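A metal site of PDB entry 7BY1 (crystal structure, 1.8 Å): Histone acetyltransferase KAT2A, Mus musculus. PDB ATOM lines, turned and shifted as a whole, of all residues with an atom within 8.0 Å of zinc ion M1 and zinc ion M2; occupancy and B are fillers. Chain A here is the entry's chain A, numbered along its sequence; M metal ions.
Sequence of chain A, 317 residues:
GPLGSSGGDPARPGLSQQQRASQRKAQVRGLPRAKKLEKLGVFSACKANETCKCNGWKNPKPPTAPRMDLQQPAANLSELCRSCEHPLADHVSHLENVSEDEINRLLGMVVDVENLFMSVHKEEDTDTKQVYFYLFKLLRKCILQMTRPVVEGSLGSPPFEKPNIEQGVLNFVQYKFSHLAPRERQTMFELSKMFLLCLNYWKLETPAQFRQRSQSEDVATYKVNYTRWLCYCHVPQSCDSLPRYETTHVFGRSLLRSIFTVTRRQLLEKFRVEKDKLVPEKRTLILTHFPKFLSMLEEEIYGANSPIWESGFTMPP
NZ of Lys 47 lies within hydrogen-bond range of O of His 91.
O of Pro 87 lies within hydrogen-bond range of ND1 of His 91, 2.8 Å away.
The backbone NH (N) of Cys 81 sits at hydrogen-bond distance from the backbone carbonyl oxygen (O) of His 86 (2.9 Å).
N of Cys 54 lies close to SG of Cys 52.
SG of Cys 54 sits close to O of Gly 56.
N of Ala 48 lies close to SG of Cys 46, 3.4 Å away.
O of Gly 56 sits close to SG of Cys 81, 3.7 Å away.
The backbone NH (N) of Gly 56 lies close to the backbone carbonyl oxygen (O) of Ser 44.
Gly 56 touches zinc ion M1 (O to ZN, 3.7 Å).
Of the 26 residues printed, 5 come within 4 Å of zinc ion M1.
The nearest printed residue that does not touch zinc ion M1 is Trp 57 (4.3 Å).
Of the 26 residues printed, 4 come within 4 Å of zinc ion M2.
Zinc ion M1 is bound by NE2 of His 91 (2.2 Å), SG of Cys 54 (2.2 Å), SG of Cys 81 (2.3 Å) and SG of Cys 84 (2.5 Å).
Zinc ion M2 is bound by a ring nitrogen (ND1) of His 86, 2.2 Å away.
SG of Cys 52 binds zinc ion M2.
SG of Cys 46 is bound to zinc ion M2, at 2.3 Å.
Zinc ion M2 is bound by SG of Cys 84.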
ATOM      1  N   GLY A  41      21.819  24.933  -7.516  1.00  0.00           N
ATOM      2  CA  GLY A  41      22.071  24.998  -8.950  1.00  0.00           C
ATOM      3  C   GLY A  41      20.887  24.531  -9.773  1.00  0.00           C
ATOM      4  O   GLY A  41      20.584  25.079 -10.841  1.00  0.00           O
ATOM      5  N   SER A  44      18.865  27.675 -10.365  1.00  0.00           N
ATOM      6  CA  SER A  44      19.638  28.889 -10.695  1.00  0.00           C
ATOM      7  C   SER A  44      19.913  29.061 -12.200  1.00  0.00           C
ATOM      8  O   SER A  44      20.160  28.096 -12.891  1.00  0.00           O
ATOM      9  CB  SER A  44      20.954  28.910  -9.936  1.00  0.00           C
ATOM     10  OG  SER A  44      20.784  28.845  -8.524  1.00  0.00           O
ATOM     11  N   ALA A  45      19.936  30.320 -12.644  1.00  0.00           N
ATOM     12  CA  ALA A  45      20.109  30.685 -14.068  1.00  0.00           C
ATOM     13  C   ALA A  45      21.509  30.425 -14.534  1.00  0.00           C
ATOM     14  O   ALA A  45      22.486  30.602 -13.803  1.00  0.00           O
ATOM     15  CB  ALA A  45      19.772  32.150 -14.287  1.00  0.00           C
ATOM     16  N   CYS A  46      21.633  29.988 -15.773  1.00  0.00           N
ATOM     17  CA  CYS A  46      22.964  29.792 -16.362  1.00  0.00           C
ATOM     18  C   CYS A  46      23.513  31.148 -16.792  1.00  0.00           C
ATOM     19  O   CYS A  46      22.785  31.917 -17.377  1.00  0.00           O
ATOM     20  CB  CYS A  46      22.900  28.828 -17.537  1.00  0.00           C
ATOM     21  SG  CYS A  46      24.563  28.450 -18.180  1.00  0.00           S
ATOM     22  N   LYS A  47      24.783  31.411 -16.496  1.00  0.00           N
ATOM     23  CA  LYS A  47      25.443  32.623 -17.003  1.00  0.00           C
ATOM     24  C   LYS A  47      26.702  32.208 -17.750  1.00  0.00           C
ATOM     25  O   LYS A  47      27.699  32.925 -17.709  1.00  0.00           O
ATOM     26  CB  LYS A  47      25.799  33.574 -15.849  1.00  0.00           C
ATOM     27  CG  LYS A  47      24.667  33.849 -14.844  1.00  0.00           C
ATOM     28  CD  LYS A  47      25.262  33.800 -13.424  1.00  0.00           C
ATOM     29  CE  LYS A  47      24.195  33.613 -12.409  1.00  0.00           C
ATOM     30  NZ  LYS A  47      23.721  32.230 -12.199  1.00  0.00           N
ATOM     31  N   ALA A  48      26.706  31.039 -18.380  1.00  0.00           N
ATOM     32  CA  ALA A  48      27.868  30.648 -19.224  1.00  0.00           C
ATOM     33  C   ALA A  48      28.207  31.702 -20.302  1.00  0.00           C
ATOM     34  O   ALA A  48      29.391  31.886 -20.628  1.00  0.00           O
ATOM     35  CB  ALA A  48      27.600  29.332 -19.898  1.00  0.00           C
ATOM     36  N   ASN A  49      27.179  32.351 -20.852  1.00  0.00           N
ATOM     37  CA  ASN A  49      27.355  33.361 -21.900  1.00  0.00           C
ATOM     38  C   ASN A  49      26.124  34.237 -21.894  1.00  0.00           C
ATOM     39  O   ASN A  49      25.159  33.933 -21.181  1.00  0.00           O
ATOM     40  CB  ASN A  49      27.569  32.712 -23.294  1.00  0.00           C
ATOM     41  CG  ASN A  49      26.446  31.757 -23.707  1.00  0.00           C
ATOM     42  OD1 ASN A  49      25.288  32.159 -23.804  1.00  0.00           O
ATOM     43  ND2 ASN A  49      26.786  30.517 -23.983  1.00  0.00           N
ATOM     44  N   THR A  51      23.790  34.579 -24.087  1.00  0.00           N
ATOM     45  CA  THR A  51      22.604  34.050 -24.798  1.00  0.00           C
ATOM     46  C   THR A  51      21.869  32.838 -24.134  1.00  0.00           C
ATOM     47  O   THR A  51      20.704  32.606 -24.418  1.00  0.00           O
ATOM     48  CB  THR A  51      22.940  33.660 -26.264  1.00  0.00           C
ATOM     49  OG1 THR A  51      23.814  32.527 -26.280  1.00  0.00           O
ATOM     50  CG2 THR A  51      23.613  34.833 -27.025  1.00  0.00           C
ATOM     51  N   CYS A  52      22.570  32.067 -23.290  1.00  0.00           N
ATOM     52  CA  CYS A  52      21.938  30.874 -22.669  1.00  0.00           C
ATOM     53  C   CYS A  52      20.810  31.324 -21.762  1.00  0.00           C
ATOM     54  O   CYS A  52      21.010  32.151 -20.897  1.00  0.00           O
ATOM     55  CB  CYS A  52      22.956  30.027 -21.903  1.00  0.00           C
ATOM     56  SG  CYS A  52      22.261  28.470 -21.253  1.00  0.00           S
ATOM     57  N   LYS A  53      19.615  30.796 -21.995  1.00  0.00           N
ATOM     58  CA  LYS A  53      18.437  31.146 -21.184  1.00  0.00           C
ATOM     59  C   LYS A  53      18.033  30.039 -20.167  1.00  0.00           C
ATOM     60  O   LYS A  53      16.919  30.069 -19.652  1.00  0.00           O
ATOM     61  CB  LYS A  53      17.236  31.346 -22.116  1.00  0.00           C
ATOM     62  CG  LYS A  53      17.344  32.432 -23.206  1.00  0.00           C
ATOM     63  CD  LYS A  53      16.429  32.104 -24.400  1.00  0.00           C
ATOM     64  CE  LYS A  53      15.153  31.308 -24.032  1.00  0.00           C
ATOM     65  NZ  LYS A  53      14.250  30.987 -25.173  1.00  0.00           N
ATOM     66  N   CYS A  54      18.887  29.063 -19.913  1.00  0.00           N
ATOM     67  CA  CYS A  54      18.543  27.984 -18.972  1.00  0.00           C
ATOM     68  C   CYS A  54      18.296  28.536 -17.571  1.00  0.00           C
ATOM     69  O   CYS A  54      19.005  29.440 -17.132  1.00  0.00           O
ATOM     70  CB  CYS A  54      19.707  27.017 -18.890  1.00  0.00           C
ATOM     71  SG  CYS A  54      19.529  25.599 -17.759  1.00  0.00           S
ATOM     72  N   ASN A  55      17.267  28.011 -16.905  1.00  0.00           N
ATOM     73  CA  ASN A  55      16.847  28.504 -15.576  1.00  0.00           C
ATOM     74  C   ASN A  55      17.171  27.477 -14.475  1.00  0.00           C
ATOM     75  O   ASN A  55      16.670  27.583 -13.348  1.00  0.00           O
ATOM     76  CB  ASN A  55      15.323  28.757 -15.546  1.00  0.00           C
ATOM     77  CG  ASN A  55      14.884  29.903 -16.439  1.00  0.00           C
ATOM     78  OD1 ASN A  55      13.780  29.849 -16.997  1.00  0.00           O
ATOM     79  ND2 ASN A  55      15.718  30.955 -16.576  1.00  0.00           N
ATOM     80  N   GLY A  56      17.917  26.415 -14.802  1.00  0.00           N
ATOM     81  CA  GLY A  56      18.254  25.436 -13.774  1.00  0.00           C
ATOM     82  C   GLY A  56      19.183  24.327 -14.258  1.00  0.00           C
ATOM     83  O   GLY A  56      18.911  23.741 -15.301  1.00  0.00           O
ATOM     84  N   TRP A  57      20.259  24.040 -13.511  1.00  0.00           N
ATOM     85  CA  TRP A  57      21.163  22.939 -13.832  1.00  0.00           C
ATOM     86  C   TRP A  57      20.476  21.616 -13.645  1.00  0.00           C
ATOM     87  O   TRP A  57      20.023  21.313 -12.540  1.00  0.00           O
ATOM     88  CB  TRP A  57      22.436  22.930 -12.980  1.00  0.00           C
ATOM     89  CG  TRP A  57      23.425  21.802 -13.233  1.00  0.00           C
ATOM     90  CD1 TRP A  57      24.395  21.753 -14.191  1.00  0.00           C
ATOM     91  CD2 TRP A  57      23.611  20.653 -12.434  1.00  0.00           C
ATOM     92  NE1 TRP A  57      25.118  20.605 -14.087  1.00  0.00           N
ATOM     93  CE2 TRP A  57      24.683  19.907 -13.007  1.00  0.00           C
ATOM     94  CE3 TRP A  57      22.976  20.145 -11.316  1.00  0.00           C
ATOM     95  CZ2 TRP A  57      25.108  18.708 -12.510  1.00  0.00           C
ATOM     96  CZ3 TRP A  57      23.406  18.964 -10.768  1.00  0.00           C
ATOM     97  CH2 TRP A  57      24.493  18.246 -11.353  1.00  0.00           C
ATOM     98  N   LYS A  58      20.486  20.810 -14.720  1.00  0.00           N
ATOM     99  CA  LYS A  58      19.920  19.428 -14.661  1.00  0.00           C
ATOM    100  C   LYS A  58      20.982  18.377 -14.678  1.00  0.00           C
ATOM    101  O   LYS A  58      21.725  18.254 -15.630  1.00  0.00           O
ATOM    102  CB  LYS A  58      18.934  19.220 -15.829  1.00  0.00           C
ATOM    103  CG  LYS A  58      17.748  20.174 -15.840  1.00  0.00           C
ATOM    104  CD  LYS A  58      16.753  19.810 -14.733  1.00  0.00           C
ATOM    105  CE  LYS A  58      15.755  20.933 -14.472  1.00  0.00           C
ATOM    106  NZ  LYS A  58      14.738  21.018 -15.552  1.00  0.00           N
ATOM    107  N   LEU A  80      28.080  18.770 -16.836  1.00  0.00           N
ATOM    108  CA  LEU A  80      27.363  19.585 -17.823  1.00  0.00           C
ATOM    109  C   LEU A  80      25.843  19.410 -17.702  1.00  0.00           C
ATOM    110  O   LEU A  80      25.361  18.304 -17.715  1.00  0.00           O
ATOM    111  CB  LEU A  80      27.794  19.173 -19.228  1.00  0.00           C
ATOM    112  CG  LEU A  80      29.284  19.353 -19.577  1.00  0.00           C
ATOM    113  CD1 LEU A  80      29.537  18.984 -21.044  1.00  0.00           C
ATOM    114  CD2 LEU A  80      29.806  20.751 -19.351  1.00  0.00           C
ATOM    115  N   CYS A  81      25.127  20.516 -17.660  1.00  0.00           N
ATOM    116  CA  CYS A  81      23.698  20.556 -17.594  1.00  0.00           C
ATOM    117  C   CYS A  81      23.067  19.736 -18.763  1.00  0.00           C
ATOM    118  O   CYS A  81      23.410  19.981 -19.925  1.00  0.00           O
ATOM    119  CB  CYS A  81      23.251  21.996 -17.724  1.00  0.00           C
ATOM    120  SG  CYS A  81      21.478  22.395 -17.565  1.00  0.00           S
ATOM    121  N   ARG A  82      22.172  18.791 -18.444  1.00  0.00           N
ATOM    122  CA  ARG A  82      21.362  18.124 -19.515  1.00  0.00           C
ATOM    123  C   ARG A  82      20.703  19.092 -20.491  1.00  0.00           C
ATOM    124  O   ARG A  82      20.568  18.790 -21.679  1.00  0.00           O
ATOM    125  CB  ARG A  82      20.196  17.335 -18.959  1.00  0.00           C
ATOM    126  CG  ARG A  82      20.568  16.046 -18.370  1.00  0.00           C
ATOM    127  CD  ARG A  82      19.332  15.220 -18.136  1.00  0.00           C
ATOM    128  NE  ARG A  82      19.625  14.254 -17.115  1.00  0.00           N
ATOM    129  CZ  ARG A  82      18.932  13.157 -16.831  1.00  0.00           C
ATOM    130  NH1 ARG A  82      17.869  12.840 -17.537  1.00  0.00           N
ATOM    131  NH2 ARG A  82      19.317  12.396 -15.822  1.00  0.00           N
ATOM    132  N   SER A  83      20.180  20.218 -19.996  1.00  0.00           N
ATOM    133  CA  SER A  83      19.439  21.130 -20.869  1.00  0.00           C
ATOM    134  C   SER A  83      20.307  21.976 -21.756  1.00  0.00           C
ATOM    135  O   SER A  83      19.989  22.169 -22.943  1.00  0.00           O
ATOM    136  CB  SER A  83      18.566  22.098 -20.047  1.00  0.00           C
ATOM    137  OG  SER A  83      17.773  21.405 -19.107  1.00  0.00           O
ATOM    138  N   CYS A  84      21.356  22.553 -21.184  1.00  0.00           N
ATOM    139  CA  CYS A  84      22.087  23.622 -21.871  1.00  0.00           C
ATOM    140  C   CYS A  84      23.547  23.250 -22.106  1.00  0.00           C
ATOM    141  O   CYS A  84      24.261  24.013 -22.757  1.00  0.00           O
ATOM    142  CB  CYS A  84      21.946  24.950 -21.068  1.00  0.00           C
ATOM    143  SG  CYS A  84      23.045  25.197 -19.643  1.00  0.00           S
ATOM    144  N   GLU A  85      23.989  22.101 -21.583  1.00  0.00           N
ATOM    145  CA  GLU A  85      25.364  21.603 -21.713  1.00  0.00           C
ATOM    146  C   GLU A  85      26.496  22.543 -21.207  1.00  0.00           C
ATOM    147  O   GLU A  85      27.647  22.462 -21.664  1.00  0.00           O
ATOM    148  CB  GLU A  85      25.597  21.109 -23.176  1.00  0.00           C
ATOM    149  CG  GLU A  85      24.528  20.103 -23.605  1.00  0.00           C
ATOM    150  CD  GLU A  85      24.842  18.637 -23.295  1.00  0.00           C
ATOM    151  OE1 GLU A  85      25.699  18.326 -22.421  1.00  0.00           O
ATOM    152  OE2 GLU A  85      24.235  17.767 -24.003  1.00  0.00           O
ATOM    153  N   HIS A  86      26.174  23.384 -20.213  1.00  0.00           N
ATOM    154  CA  HIS A  86      27.141  24.227 -19.572  1.00  0.00           C
ATOM    155  C   HIS A  86      27.340  23.687 -18.166  1.00  0.00           C
ATOM    156  O   HIS A  86      26.432  23.077 -17.575  1.00  0.00           O
ATOM    157  CB  HIS A  86      26.738  25.693 -19.613  1.00  0.00           C
ATOM    158  CG  HIS A  86      26.617  26.243 -21.005  1.00  0.00           C
ATOM    159  ND1 HIS A  86      25.496  26.926 -21.444  1.00  0.00           N
ATOM    160  CD2 HIS A  86      27.456  26.174 -22.081  1.00  0.00           C
ATOM    161  CE1 HIS A  86      25.664  27.322 -22.703  1.00  0.00           C
ATOM    162  NE2 HIS A  86      26.840  26.852 -23.115  1.00  0.00           N
ATOM    163  N   PRO A  87      28.528  23.876 -17.603  1.00  0.00           N
ATOM    164  CA  PRO A  87      28.809  23.253 -16.315  1.00  0.00           C
ATOM    165  C   PRO A  87      27.902  23.819 -15.177  1.00  0.00           C
ATOM    166  O   PRO A  87      27.417  24.960 -15.301  1.00  0.00           O
ATOM    167  CB  PRO A  87      30.254  23.691 -16.024  1.00  0.00           C
ATOM    168  CG  PRO A  87      30.860  23.933 -17.351  1.00  0.00           C
ATOM    169  CD  PRO A  87      29.764  24.415 -18.244  1.00  0.00           C
ATOM    170  N   LEU A  88      27.742  23.024 -14.141  1.00  0.00           N
ATOM    171  CA  LEU A  88      27.109  23.471 -12.854  1.00  0.00           C
ATOM    172  C   LEU A  88      27.758  24.799 -12.408  1.00  0.00           C
ATOM    173  O   LEU A  88      27.038  25.727 -12.062  1.00  0.00           O
ATOM    174  CB  LEU A  88      27.222  22.381 -11.801  1.00  0.00           C
ATOM    175  CG  LEU A  88      26.850  22.686 -10.346  1.00  0.00           C
ATOM    176  CD1 LEU A  88      25.428  23.189 -10.256  1.00  0.00           C
ATOM    177  CD2 LEU A  88      27.087  21.466  -9.499  1.00  0.00           C
ATOM    178  N   ASP A  90      28.709  27.328 -13.979  1.00  0.00           N
ATOM    179  CA  ASP A  90      28.157  28.508 -14.609  1.00  0.00           C
ATOM    180  C   ASP A  90      26.720  28.857 -14.119  1.00  0.00           C
ATOM    181  O   ASP A  90      26.223  29.917 -14.434  1.00  0.00           O
ATOM    182  CB  ASP A  90      28.148  28.387 -16.110  1.00  0.00           C
ATOM    183  CG  ASP A  90      29.556  28.187 -16.728  1.00  0.00           C
ATOM    184  OD1 ASP A  90      30.569  28.568 -16.155  1.00  0.00           O
ATOM    185  OD2 ASP A  90      29.593  27.651 -17.838  1.00  0.00           O
ATOM    186  N   HIS A  91      26.055  27.894 -13.477  1.00  0.00           N
ATOM    187  CA  HIS A  91      24.711  28.127 -12.927  1.00  0.00           C
ATOM    188  C   HIS A  91      24.805  28.650 -11.465  1.00  0.00           C
ATOM    189  O   HIS A  91      23.869  29.326 -11.035  1.00  0.00           O
ATOM    190  CB  HIS A  91      23.891  26.830 -12.934  1.00  0.00           C
ATOM    191  CG  HIS A  91      23.685  26.253 -14.314  1.00  0.00           C
ATOM    192  ND1 HIS A  91      24.707  25.664 -15.046  1.00  0.00           N
ATOM    193  CD2 HIS A  91      22.557  26.095 -15.044  1.00  0.00           C
ATOM    194  CE1 HIS A  91      24.215  25.192 -16.178  1.00  0.00           C
ATOM    195  NE2 HIS A  91      22.918  25.444 -16.202  1.00  0.00           N
HETATM  196 ZN    ZN M   1      21.563  24.672 -17.743  1.00  0.00          ZN
HETATM  197 ZN    ZN M   2      23.817  27.401 -20.052  1.00  0.00          ZN
